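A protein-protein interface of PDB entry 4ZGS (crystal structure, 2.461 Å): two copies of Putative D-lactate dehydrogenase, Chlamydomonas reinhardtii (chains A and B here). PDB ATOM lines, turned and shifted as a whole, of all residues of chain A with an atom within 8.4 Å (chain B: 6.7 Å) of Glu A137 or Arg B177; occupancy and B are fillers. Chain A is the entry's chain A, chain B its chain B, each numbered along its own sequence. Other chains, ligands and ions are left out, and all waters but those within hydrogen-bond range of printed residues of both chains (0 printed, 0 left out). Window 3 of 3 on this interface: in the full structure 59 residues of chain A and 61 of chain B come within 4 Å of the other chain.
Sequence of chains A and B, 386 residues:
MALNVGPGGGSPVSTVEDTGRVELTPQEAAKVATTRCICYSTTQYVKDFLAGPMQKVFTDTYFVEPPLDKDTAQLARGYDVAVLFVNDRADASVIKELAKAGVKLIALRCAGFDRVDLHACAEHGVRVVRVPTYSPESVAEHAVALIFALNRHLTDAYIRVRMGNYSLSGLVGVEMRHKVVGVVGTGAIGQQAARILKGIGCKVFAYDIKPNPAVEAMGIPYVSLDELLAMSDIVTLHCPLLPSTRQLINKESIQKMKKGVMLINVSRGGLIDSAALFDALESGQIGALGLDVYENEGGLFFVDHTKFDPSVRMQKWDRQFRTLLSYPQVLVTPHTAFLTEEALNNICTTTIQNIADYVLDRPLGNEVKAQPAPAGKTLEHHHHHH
The side-chain carboxylate (OE2) of Glu B175 sits close to the side-chain hydroxyl (OG) of Ser A135. The side-chain carboxylate (OE2) of Glu A137 is in salt-bridge range of the guanidinium group (NH1) of Arg B177 (2.9 Å). The guanidinium group of Arg B152 sits at hydrogen-bond distance from the backbone carbonyl oxygen of Ser A138. OE2 of Glu B175 is in hydrogen-bond range of OG of Ser A138. The side-chain carboxylate (OE1) of Glu A141 lies within hydrogen-bond range of the backbone NH (N) of Met B176, at 2.6 Å. OE2 of Glu A141 lies within hydrogen-bond range of N of Arg B177. ND1 of His A142 lies within hydrogen-bond range of NH2 of Arg B152 (3.2 Å). The side-chain amide oxygen (OE1) of Gln A192 is in hydrogen-bond range of the guanidinium group (NH1) of Arg B177 (3.3 Å). The backbone carbonyl oxygen (O) of Ile B200 sits at hydrogen-bond distance from the guanidinium group (NH2) of Arg A195 (3.0 Å). The backbone carbonyl oxygen (O) of Ala A337 lies within hydrogen-bond range of the guanidinium group (NH2) of Arg B152, 2.7 Å away. N of Glu B175 sits at hydrogen-bond distance from OE1 of Glu A342 (3.0 Å). OE2 of Glu A342 is in salt-bridge range of NZ of Lys B179.
OG of Ser A135 sits at hydrogen-bond distance from OD1 of Asn A346 (2.8 Å). OG of Ser A138 lies close to OG1 of Thr A340 (3.4 Å). N of Val A139 sits close to O of Ala A337, 3.5 Å away. The side-chain amide oxygen (OE1) of Gln A192 lies within hydrogen-bond range of the guanidinium group (NE) of Arg A195, 2.7 Å away. The side-chain sulfur (SG) of Cys B202 is in hydrogen-bond range of the backbone carbonyl oxygen (O) of Met B176 (3.4 Å). The backbone carbonyl oxygen of Lys B179 sits at hydrogen-bond distance from the backbone NH of Lys B203, at 2.9 Å.
Glu A137 touches Glu B175. Arg B152 touches Glu A141 (NH1 to CB, 3.95 Å). OE1 of Glu A141 touches CA of Glu B175, at 3.3 Å. Arg A195 touches Arg B177. CZ of Arg B152 touches OG1 of Thr A340, at 3.8 Å. Thr A340 touches Val B174 (OG1 to N, 3.8 Å). Thr A340 touches Glu B175. Glu A342 touches Val B174 (OE1 to CA, 3.9 Å).
Glu A137 touches just these residues of chain B: Glu B175 and Arg B177. Of chain A, only Glu A137, Glu A141, Gln A192 and Arg A195 come within 4 Å of Arg B177. Of the printed residues of chain B, Gln A192 touches Arg B177 (3.3 Å). Printed residues of chain B within 4 Å of Arg A195: Arg B177 (3.5 Å) and Ile B200 (3.0 Å). Printed residues of chain B within 4 Å of Ser A138: Arg B152 (2.6 Å) and Glu B175 (2.8 Å). Printed residues of chain B within 4 Å of Glu A141: Arg B152, Glu B175, Met B176 and Arg B177. The nearest residue of chain B that does not touch Glu A137 is Arg B152 (4.9 Å). The nearest printed residue of chain B that does not touch Ser A138 is Val B174 (5.9 Å).
Printed residues of chain B that touch a printed residue of chain A: Arg B152, Val B174, Glu B175, Met B176, Arg B177, Lys B179 and Ile B200. Among the printed residues, 20 pairs touch across the chains.
No position is printed for both chains.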
ATOM      1  N   TYR A 134      31.908  -9.603 -21.717  1.00  0.00           N
ATOM      2  CA  TYR A 134      31.975  -8.844 -20.470  1.00  0.00           C
ATOM      3  C   TYR A 134      30.810  -7.834 -20.422  1.00  0.00           C
ATOM      4  O   TYR A 134      30.276  -7.479 -21.469  1.00  0.00           O
ATOM      5  CB  TYR A 134      33.308  -8.093 -20.354  1.00  0.00           C
ATOM      6  CG  TYR A 134      34.509  -8.813 -20.923  1.00  0.00           C
ATOM      7  CD1 TYR A 134      34.703 -10.176 -20.730  1.00  0.00           C
ATOM      8  CD2 TYR A 134      35.454  -8.120 -21.661  1.00  0.00           C
ATOM      9  CE1 TYR A 134      35.818 -10.831 -21.266  1.00  0.00           C
ATOM     10  CE2 TYR A 134      36.562  -8.754 -22.194  1.00  0.00           C
ATOM     11  CZ  TYR A 134      36.748 -10.106 -21.998  1.00  0.00           C
ATOM     12  OH  TYR A 134      37.865 -10.712 -22.541  1.00  0.00           O
ATOM     13  N   SER A 135      30.423  -7.380 -19.224  1.00  0.00           N
ATOM     14  CA  SER A 135      29.422  -6.310 -19.085  1.00  0.00           C
ATOM     15  C   SER A 135      29.814  -5.062 -19.843  1.00  0.00           C
ATOM     16  O   SER A 135      30.802  -4.439 -19.532  1.00  0.00           O
ATOM     17  CB  SER A 135      29.224  -5.901 -17.621  1.00  0.00           C
ATOM     18  OG  SER A 135      28.931  -7.000 -16.793  1.00  0.00           O
ATOM     19  N   PRO A 136      29.016  -4.681 -20.829  1.00  0.00           N
ATOM     20  CA  PRO A 136      29.339  -3.577 -21.734  1.00  0.00           C
ATOM     21  C   PRO A 136      29.371  -2.244 -20.969  1.00  0.00           C
ATOM     22  O   PRO A 136      30.024  -1.291 -21.402  1.00  0.00           O
ATOM     23  CB  PRO A 136      28.193  -3.611 -22.759  1.00  0.00           C
ATOM     24  CG  PRO A 136      27.078  -4.329 -22.056  1.00  0.00           C
ATOM     25  CD  PRO A 136      27.746  -5.338 -21.171  1.00  0.00           C
ATOM     26  N   GLU A 137      28.666  -2.183 -19.842  1.00  0.00           N
ATOM     27  CA  GLU A 137      28.768  -1.027 -18.962  1.00  0.00           C
ATOM     28  C   GLU A 137      30.169  -0.818 -18.424  1.00  0.00           C
ATOM     29  O   GLU A 137      30.623   0.327 -18.321  1.00  0.00           O
ATOM     30  CB  GLU A 137      27.806  -1.144 -17.779  1.00  0.00           C
ATOM     31  CG  GLU A 137      26.396  -0.842 -18.112  1.00  0.00           C
ATOM     32  CD  GLU A 137      25.685  -2.031 -18.643  1.00  0.00           C
ATOM     33  OE1 GLU A 137      26.375  -3.063 -18.866  1.00  0.00           O
ATOM     34  OE2 GLU A 137      24.454  -1.896 -18.885  1.00  0.00           O
ATOM     35  N   SER A 138      30.843  -1.906 -18.044  1.00  0.00           N
ATOM     36  CA  SER A 138      32.188  -1.791 -17.461  1.00  0.00           C
ATOM     37  C   SER A 138      33.123  -1.054 -18.387  1.00  0.00           C
ATOM     38  O   SER A 138      33.795  -0.111 -17.966  1.00  0.00           O
ATOM     39  CB  SER A 138      32.777  -3.153 -17.127  1.00  0.00           C
ATOM     40  OG  SER A 138      32.221  -3.671 -15.934  1.00  0.00           O
ATOM     41  N   VAL A 139      33.137  -1.484 -19.648  1.00  0.00           N
ATOM     42  CA  VAL A 139      34.046  -0.945 -20.650  1.00  0.00           C
ATOM     43  C   VAL A 139      33.651   0.484 -20.994  1.00  0.00           C
ATOM     44  O   VAL A 139      34.482   1.400 -20.936  1.00  0.00           O
ATOM     45  CB  VAL A 139      34.080  -1.876 -21.914  1.00  0.00           C
ATOM     46  CG1 VAL A 139      34.972  -1.328 -22.998  1.00  0.00           C
ATOM     47  CG2 VAL A 139      34.516  -3.277 -21.524  1.00  0.00           C
ATOM     48  N   ALA A 140      32.360   0.705 -21.254  1.00  0.00           N
ATOM     49  CA  ALA A 140      31.872   2.053 -21.606  1.00  0.00           C
ATOM     50  C   ALA A 140      32.128   3.021 -20.456  1.00  0.00           C
ATOM     51  O   ALA A 140      32.526   4.127 -20.681  1.00  0.00           O
ATOM     52  CB  ALA A 140      30.400   2.036 -21.951  1.00  0.00           C
ATOM     53  N   GLU A 141      31.880   2.614 -19.219  1.00  0.00           N
ATOM     54  CA  GLU A 141      32.168   3.496 -18.106  1.00  0.00           C
ATOM     55  C   GLU A 141      33.700   3.764 -17.998  1.00  0.00           C
ATOM     56  O   GLU A 141      34.107   4.746 -17.408  1.00  0.00           O
ATOM     57  CB  GLU A 141      31.631   2.905 -16.806  1.00  0.00           C
ATOM     58  CG  GLU A 141      30.104   2.833 -16.781  1.00  0.00           C
ATOM     59  CD  GLU A 141      29.525   2.257 -15.501  1.00  0.00           C
ATOM     60  OE1 GLU A 141      30.293   1.916 -14.576  1.00  0.00           O
ATOM     61  OE2 GLU A 141      28.285   2.164 -15.419  1.00  0.00           O
ATOM     62  N   HIS A 142      34.547   2.891 -18.544  1.00  0.00           N
ATOM     63  CA  HIS A 142      35.967   3.138 -18.399  1.00  0.00           C
ATOM     64  C   HIS A 142      36.453   4.252 -19.321  1.00  0.00           C
ATOM     65  O   HIS A 142      37.223   5.117 -18.911  1.00  0.00           O
ATOM     66  CB  HIS A 142      36.768   1.867 -18.643  1.00  0.00           C
ATOM     67  CG  HIS A 142      38.201   1.995 -18.259  1.00  0.00           C
ATOM     68  ND1 HIS A 142      38.610   1.936 -16.944  1.00  0.00           N
ATOM     69  CD2 HIS A 142      39.327   2.125 -19.002  1.00  0.00           C
ATOM     70  CE1 HIS A 142      39.922   2.062 -16.891  1.00  0.00           C
ATOM     71  NE2 HIS A 142      40.377   2.188 -18.126  1.00  0.00           N
ATOM     72  N   ALA A 143      36.002   4.216 -20.567  1.00  0.00           N
ATOM     73  CA  ALA A 143      36.273   5.295 -21.501  1.00  0.00           C
ATOM     74  C   ALA A 143      35.766   6.643 -20.961  1.00  0.00           C
ATOM     75  O   ALA A 143      36.426   7.695 -21.115  1.00  0.00           O
ATOM     76  CB  ALA A 143      35.647   4.996 -22.831  1.00  0.00           C
ATOM     77  N   VAL A 144      34.595   6.610 -20.329  1.00  0.00           N
ATOM     78  CA  VAL A 144      34.004   7.827 -19.797  1.00  0.00           C
ATOM     79  C   VAL A 144      34.891   8.272 -18.628  1.00  0.00           C
ATOM     80  O   VAL A 144      35.065   9.462 -18.368  1.00  0.00           O
ATOM     81  CB  VAL A 144      32.519   7.614 -19.356  1.00  0.00           C
ATOM     82  CG1 VAL A 144      31.944   8.884 -18.776  1.00  0.00           C
ATOM     83  CG2 VAL A 144      31.697   7.219 -20.548  1.00  0.00           C
ATOM     84  N   ALA A 188      27.380  -3.356 -28.570  1.00  0.00           N
ATOM     85  CA  ALA A 188      27.003  -3.455 -27.163  1.00  0.00           C
ATOM     86  C   ALA A 188      27.707  -2.408 -26.289  1.00  0.00           C
ATOM     87  O   ALA A 188      27.072  -1.736 -25.480  1.00  0.00           O
ATOM     88  CB  ALA A 188      27.300  -4.859 -26.655  1.00  0.00           C
ATOM     89  N   ILE A 189      29.011  -2.246 -26.479  1.00  0.00           N
ATOM     90  CA  ILE A 189      29.788  -1.259 -25.728  1.00  0.00           C
ATOM     91  C   ILE A 189      29.582   0.214 -26.178  1.00  0.00           C
ATOM     92  O   ILE A 189      29.321   1.092 -25.346  1.00  0.00           O
ATOM     93  CB  ILE A 189      31.275  -1.610 -25.823  1.00  0.00           C
ATOM     94  CG1 ILE A 189      31.526  -2.905 -25.047  1.00  0.00           C
ATOM     95  CG2 ILE A 189      32.115  -0.509 -25.278  1.00  0.00           C
ATOM     96  CD1 ILE A 189      32.867  -3.562 -25.316  1.00  0.00           C
ATOM     97  N   GLY A 190      29.691   0.473 -27.483  1.00  0.00           N
ATOM     98  CA  GLY A 190      29.439   1.805 -28.019  1.00  0.00           C
ATOM     99  C   GLY A 190      28.037   2.308 -27.655  1.00  0.00           C
ATOM    100  O   GLY A 190      27.862   3.486 -27.289  1.00  0.00           O
ATOM    101  N   GLN A 191      27.056   1.407 -27.689  1.00  0.00           N
ATOM    102  CA  GLN A 191      25.696   1.756 -27.271  1.00  0.00           C
ATOM    103  C   GLN A 191      25.690   2.304 -25.844  1.00  0.00           C
ATOM    104  O   GLN A 191      24.990   3.299 -25.559  1.00  0.00           O
ATOM    105  CB  GLN A 191      24.755   0.546 -27.385  1.00  0.00           C
ATOM    106  CG  GLN A 191      23.309   0.811 -27.017  1.00  0.00           C
ATOM    107  CD  GLN A 191      22.474  -0.461 -27.079  1.00  0.00           C
ATOM    108  OE1 GLN A 191      22.669  -1.297 -27.956  1.00  0.00           O
ATOM    109  NE2 GLN A 191      21.575  -0.628 -26.129  1.00  0.00           N
ATOM    110  N   GLN A 192      26.438   1.659 -24.945  1.00  0.00           N
ATOM    111  CA  GLN A 192      26.496   2.130 -23.568  1.00  0.00           C
ATOM    112  C   GLN A 192      27.260   3.458 -23.491  1.00  0.00           C
ATOM    113  O   GLN A 192      26.920   4.323 -22.684  1.00  0.00           O
ATOM    114  CB  GLN A 192      27.132   1.092 -22.642  1.00  0.00           C
ATOM    115  CG  GLN A 192      26.310  -0.187 -22.491  1.00  0.00           C
ATOM    116  CD  GLN A 192      24.847   0.107 -22.104  1.00  0.00           C
ATOM    117  OE1 GLN A 192      24.571   0.998 -21.309  1.00  0.00           O
ATOM    118  NE2 GLN A 192      23.922  -0.629 -22.686  1.00  0.00           N
ATOM    119  N   ALA A 193      28.267   3.632 -24.341  1.00  0.00           N
ATOM    120  CA  ALA A 193      29.079   4.841 -24.253  1.00  0.00           C
ATOM    121  C   ALA A 193      28.204   5.999 -24.666  1.00  0.00           C
ATOM    122  O   ALA A 193      28.169   7.034 -24.017  1.00  0.00           O
ATOM    123  CB  ALA A 193      30.347   4.738 -25.119  1.00  0.00           C
ATOM    124  N   ARG A 195      24.850   6.016 -24.496  1.00  0.00           N
ATOM    125  CA  ARG A 195      23.851   6.224 -23.443  1.00  0.00           C
ATOM    126  C   ARG A 195      24.417   7.095 -22.320  1.00  0.00           C
ATOM    127  O   ARG A 195      23.802   8.089 -21.939  1.00  0.00           O
ATOM    128  CB  ARG A 195      23.361   4.896 -22.850  1.00  0.00           C
ATOM    129  CG  ARG A 195      22.355   5.095 -21.709  1.00  0.00           C
ATOM    130  CD  ARG A 195      21.965   3.801 -20.982  1.00  0.00           C
ATOM    131  NE  ARG A 195      23.128   3.123 -20.382  1.00  0.00           N
ATOM    132  CZ  ARG A 195      23.729   3.526 -19.257  1.00  0.00           C
ATOM    133  NH1 ARG A 195      24.783   2.866 -18.781  1.00  0.00           N
ATOM    134  NH2 ARG A 195      23.300   4.613 -18.622  1.00  0.00           N
ATOM    135  N   ILE A 196      25.582   6.713 -21.788  1.00  0.00           N
ATOM    136  CA  ILE A 196      26.229   7.443 -20.687  1.00  0.00           C
ATOM    137  C   ILE A 196      26.574   8.891 -21.061  1.00  0.00           C
ATOM    138  O   ILE A 196      26.305   9.846 -20.296  1.00  0.00           O
ATOM    139  CB  ILE A 196      27.539   6.737 -20.230  1.00  0.00           C
ATOM    140  CG1 ILE A 196      27.273   5.361 -19.613  1.00  0.00           C
ATOM    141  CG2 ILE A 196      28.246   7.570 -19.201  1.00  0.00           C
ATOM    142  CD1 ILE A 196      28.536   4.425 -19.598  1.00  0.00           C
ATOM    143  N   ALA A 337      39.779  -1.785 -18.763  1.00  0.00           N
ATOM    144  CA  ALA A 337      38.406  -1.373 -19.025  1.00  0.00           C
ATOM    145  C   ALA A 337      37.366  -2.463 -18.683  1.00  0.00           C
ATOM    146  O   ALA A 337      36.257  -2.118 -18.298  1.00  0.00           O
ATOM    147  CB  ALA A 337      38.232  -0.934 -20.485  1.00  0.00           C
ATOM    148  N   PHE A 338      37.719  -3.741 -18.851  1.00  0.00           N
ATOM    149  CA  PHE A 338      36.814  -4.845 -18.531  1.00  0.00           C
ATOM    150  C   PHE A 338      36.944  -5.202 -17.075  1.00  0.00           C
ATOM    151  O   PHE A 338      36.206  -6.030 -16.566  1.00  0.00           O
ATOM    152  CB  PHE A 338      37.116  -6.113 -19.323  1.00  0.00           C
ATOM    153  CG  PHE A 338      38.252  -6.934 -18.717  1.00  0.00           C
ATOM    154  CD1 PHE A 338      39.558  -6.438 -18.702  1.00  0.00           C
ATOM    155  CD2 PHE A 338      38.008  -8.153 -18.097  1.00  0.00           C
ATOM    156  CE1 PHE A 338      40.612  -7.191 -18.123  1.00  0.00           C
ATOM    157  CE2 PHE A 338      39.050  -8.897 -17.513  1.00  0.00           C
ATOM    158  CZ  PHE A 338      40.351  -8.415 -17.530  1.00  0.00           C
ATOM    159  N   THR A 340      36.423  -5.258 -13.587  1.00  0.00           N
ATOM    160  CA  THR A 340      35.390  -4.762 -12.712  1.00  0.00           C
ATOM    161  C   THR A 340      34.882  -5.921 -11.888  1.00  0.00           C
ATOM    162  O   THR A 340      34.922  -7.029 -12.360  1.00  0.00           O
ATOM    163  CB  THR A 340      34.284  -4.123 -13.568  1.00  0.00           C
ATOM    164  OG1 THR A 340      34.536  -2.704 -13.656  1.00  0.00           O
ATOM    165  CG2 THR A 340      32.909  -4.386 -13.003  1.00  0.00           C
ATOM    166  N   GLU A 342      31.758  -6.569 -11.295  1.00  0.00           N
ATOM    167  CA  GLU A 342      30.613  -7.068 -12.085  1.00  0.00           C
ATOM    168  C   GLU A 342      31.035  -7.875 -13.325  1.00  0.00           C
ATOM    169  O   GLU A 342      30.422  -8.901 -13.620  1.00  0.00           O
ATOM    170  CB  GLU A 342      29.668  -5.923 -12.506  1.00  0.00           C
ATOM    171  CG  GLU A 342      28.951  -5.208 -11.331  1.00  0.00           C
ATOM    172  CD  GLU A 342      29.799  -4.096 -10.649  1.00  0.00           C
ATOM    173  OE1 GLU A 342      30.957  -3.906 -11.050  1.00  0.00           O
ATOM    174  OE2 GLU A 342      29.302  -3.407  -9.726  1.00  0.00           O
ATOM    175  N   ALA A 343      32.032  -7.401 -14.074  1.00  0.00           N
ATOM    176  CA  ALA A 343      32.449  -8.121 -15.277  1.00  0.00           C
ATOM    177  C   ALA A 343      33.128  -9.470 -14.953  1.00  0.00           C
ATOM    178  O   ALA A 343      32.917 -10.450 -15.663  1.00  0.00           O
ATOM    179  CB  ALA A 343      33.354  -7.273 -16.123  1.00  0.00           C
ATOM    180  N   ASN A 346      30.508 -12.214 -14.236  1.00  0.00           N
ATOM    181  CA  ASN A 346      30.046 -12.787 -15.486  1.00  0.00           C
ATOM    182  C   ASN A 346      31.049 -13.831 -15.965  1.00  0.00           C
ATOM    183  O   ASN A 346      30.694 -14.971 -16.296  1.00  0.00           O
ATOM    184  CB  ASN A 346      29.889 -11.709 -16.568  1.00  0.00           C
ATOM    185  CG  ASN A 346      28.769 -10.710 -16.272  1.00  0.00           C
ATOM    186  OD1 ASN A 346      28.594  -9.733 -17.007  1.00  0.00           O
ATOM    187  ND2 ASN A 346      28.026 -10.937 -15.196  1.00  0.00           N
ATOM    188  N   ARG B 152      37.600   3.345 -10.814  1.00  0.00           N
ATOM    189  CA  ARG B 152      38.470   2.643 -11.745  1.00  0.00           C
ATOM    190  C   ARG B 152      39.960   2.749 -11.342  1.00  0.00           C
ATOM    191  O   ARG B 152      40.837   2.462 -12.146  1.00  0.00           O
ATOM    192  CB  ARG B 152      38.190   3.104 -13.175  1.00  0.00           C
ATOM    193  CG  ARG B 152      36.632   3.010 -13.574  1.00  0.00           C
ATOM    194  CD  ARG B 152      35.979   1.645 -13.270  1.00  0.00           C
ATOM    195  NE  ARG B 152      36.536   0.717 -14.230  1.00  0.00           N
ATOM    196  CZ  ARG B 152      35.961   0.327 -15.347  1.00  0.00           C
ATOM    197  NH1 ARG B 152      34.717   0.717 -15.663  1.00  0.00           N
ATOM    198  NH2 ARG B 152      36.635  -0.495 -16.138  1.00  0.00           N
ATOM    199  N   VAL B 174      34.815  -0.969 -10.264  1.00  0.00           N
ATOM    200  CA  VAL B 174      33.380  -1.088  -9.998  1.00  0.00           C
ATOM    201  C   VAL B 174      32.533  -0.356 -11.027  1.00  0.00           C
ATOM    202  O   VAL B 174      32.890   0.731 -11.535  1.00  0.00           O
ATOM    203  CB  VAL B 174      33.065  -0.575  -8.577  1.00  0.00           C
ATOM    204  CG1 VAL B 174      31.891   0.351  -8.543  1.00  0.00           C
ATOM    205  CG2 VAL B 174      32.944  -1.739  -7.610  1.00  0.00           C
ATOM    206  N   GLU B 175      31.400  -0.966 -11.343  1.00  0.00           N
ATOM    207  CA  GLU B 175      30.429  -0.355 -12.249  1.00  0.00           C
ATOM    208  C   GLU B 175      29.657   0.719 -11.520  1.00  0.00           C
ATOM    209  O   GLU B 175      29.422   0.599 -10.317  1.00  0.00           O
ATOM    210  CB  GLU B 175      29.466  -1.404 -12.812  1.00  0.00           C
ATOM    211  CG  GLU B 175      30.038  -2.137 -13.999  1.00  0.00           C
ATOM    212  CD  GLU B 175      29.049  -3.068 -14.652  1.00  0.00           C
ATOM    213  OE1 GLU B 175      27.860  -3.033 -14.244  1.00  0.00           O
ATOM    214  OE2 GLU B 175      29.479  -3.846 -15.547  1.00  0.00           O
ATOM    215  N   MET B 176      29.344   1.810 -12.205  1.00  0.00           N
ATOM    216  CA  MET B 176      28.466   2.792 -11.607  1.00  0.00           C
ATOM    217  C   MET B 176      26.994   2.624 -11.964  1.00  0.00           C
ATOM    218  O   MET B 176      26.126   3.175 -11.275  1.00  0.00           O
ATOM    219  CB  MET B 176      28.911   4.200 -11.977  1.00  0.00           C
ATOM    220  CG  MET B 176      28.916   5.124 -10.774  1.00  0.00           C
ATOM    221  SD  MET B 176      29.303   6.739 -11.370  1.00  0.00           S
ATOM    222  CE  MET B 176      30.744   6.300 -12.312  1.00  0.00           C
ATOM    223  N   ARG B 177      26.681   1.844 -12.993  1.00  0.00           N
ATOM    224  CA  ARG B 177      25.338   1.943 -13.578  1.00  0.00           C
ATOM    225  C   ARG B 177      24.147   1.861 -12.636  1.00  0.00           C
ATOM    226  O   ARG B 177      23.290   2.703 -12.705  1.00  0.00           O
ATOM    227  CB  ARG B 177      25.065   0.896 -14.649  1.00  0.00           C
ATOM    228  CG  ARG B 177      23.666   1.136 -15.237  1.00  0.00           C
ATOM    229  CD  ARG B 177      23.381   0.483 -16.598  1.00  0.00           C
ATOM    230  NE  ARG B 177      22.114   0.998 -17.115  1.00  0.00           N
ATOM    231  CZ  ARG B 177      21.600   0.730 -18.313  1.00  0.00           C
ATOM    232  NH1 ARG B 177      22.223  -0.064 -19.177  1.00  0.00           N
ATOM    233  NH2 ARG B 177      20.458   1.297 -18.660  1.00  0.00           N
ATOM    234  N   HIS B 178      23.999   0.860 -11.809  1.00  0.00           N
ATOM    235  CA  HIS B 178      22.739   0.838 -11.029  1.00  0.00           C
ATOM    236  C   HIS B 178      22.866   1.278  -9.601  1.00  0.00           C
ATOM    237  O   HIS B 178      21.977   1.016  -8.794  1.00  0.00           O
ATOM    238  CB  HIS B 178      22.106  -0.547 -11.101  1.00  0.00           C
ATOM    239  CG  HIS B 178      21.666  -0.881 -12.482  1.00  0.00           C
ATOM    240  ND1 HIS B 178      22.391  -1.710 -13.310  1.00  0.00           N
ATOM    241  CD2 HIS B 178      20.648  -0.396 -13.231  1.00  0.00           C
ATOM    242  CE1 HIS B 178      21.798  -1.782 -14.487  1.00  0.00           C
ATOM    243  NE2 HIS B 178      20.737  -0.993 -14.465  1.00  0.00           N
ATOM    244  N   LYS B 179      24.030   1.818  -9.272  1.00  0.00           N
ATOM    245  CA  LYS B 179      24.386   2.146  -7.905  1.00  0.00           C
ATOM    246  C   LYS B 179      23.502   3.217  -7.288  1.00  0.00           C
ATOM    247  O   LYS B 179      22.945   4.083  -7.986  1.00  0.00           O
ATOM    248  CB  LYS B 179      25.856   2.577  -7.856  1.00  0.00           C
ATOM    249  CG  LYS B 179      26.785   1.548  -8.469  1.00  0.00           C
ATOM    250  CD  LYS B 179      26.593   0.181  -7.792  1.00  0.00           C
ATOM    251  CE  LYS B 179      27.216  -0.983  -8.589  1.00  0.00           C
ATOM    252  NZ  LYS B 179      28.708  -1.027  -8.501  1.00  0.00           N
ATOM    253  N   LEU B 197      24.191  12.399 -12.563  1.00  0.00           N
ATOM    254  CA  LEU B 197      24.217  11.063 -12.015  1.00  0.00           C
ATOM    255  C   LEU B 197      23.035  10.223 -12.517  1.00  0.00           C
ATOM    256  O   LEU B 197      23.228   9.061 -12.892  1.00  0.00           O
ATOM    257  CB  LEU B 197      24.253  11.129 -10.488  1.00  0.00           C
ATOM    258  CG  LEU B 197      25.672  11.557 -10.059  1.00  0.00           C
ATOM    259  CD1 LEU B 197      25.753  12.169  -8.647  1.00  0.00           C
ATOM    260  CD2 LEU B 197      26.648  10.390 -10.231  1.00  0.00           C
ATOM    261  N   ILE B 200      23.797   9.128 -15.968  1.00  0.00           N
ATOM    262  CA  ILE B 200      24.766   8.025 -15.977  1.00  0.00           C
ATOM    263  C   ILE B 200      24.080   6.712 -15.733  1.00  0.00           C
ATOM    264  O   ILE B 200      24.607   5.665 -16.078  1.00  0.00           O
ATOM    265  CB  ILE B 200      25.864   8.245 -14.941  1.00  0.00           C
ATOM    266  CG1 ILE B 200      26.800   9.354 -15.447  1.00  0.00           C
ATOM    267  CG2 ILE B 200      26.663   6.991 -14.723  1.00  0.00           C
ATOM    268  CD1 ILE B 200      27.643   9.961 -14.378  1.00  0.00           C
ATOM    269  N   GLY B 201      22.871   6.769 -15.169  1.00  0.00           N
ATOM    270  CA  GLY B 201      22.122   5.556 -14.901  1.00  0.00           C
ATOM    271  C   GLY B 201      21.994   5.163 -13.440  1.00  0.00           C
ATOM    272  O   GLY B 201      21.496   4.092 -13.130  1.00  0.00           O
ATOM    273  N   CYS B 202      22.479   5.986 -12.534  1.00  0.00           N
ATOM    274  CA  CYS B 202      22.386   5.684 -11.110  1.00  0.00           C
ATOM    275  C   CYS B 202      20.980   5.842 -10.550  1.00  0.00           C
ATOM    276  O   CYS B 202      20.161   6.556 -11.104  1.00  0.00           O
ATOM    277  CB  CYS B 202      23.339   6.590 -10.329  1.00  0.00           C
ATOM    278  SG  CYS B 202      25.024   6.403 -10.936  1.00  0.00           S
ATOM    279  N   LYS B 203      20.723   5.210  -9.417  1.00  0.00           N
ATOM    280  CA  LYS B 203      19.492   5.448  -8.711  1.00  0.00           C
ATOM    281  C   LYS B 203      19.780   6.549  -7.728  1.00  0.00           C
ATOM    282  O   LYS B 203      20.369   6.307  -6.678  1.00  0.00           O
ATOM    283  CB  LYS B 203      19.029   4.177  -7.984  1.00  0.00           C
ATOM    284  CG  LYS B 203      18.943   2.989  -8.934  1.00  0.00           C
ATOM    285  CD  LYS B 203      18.640   1.654  -8.269  1.00  0.00           C
ATOM    286  CE  LYS B 203      18.630   0.589  -9.342  1.00  0.00           C
ATOM    287  NZ  LYS B 203      18.353  -0.767  -8.805  1.00  0.00           N
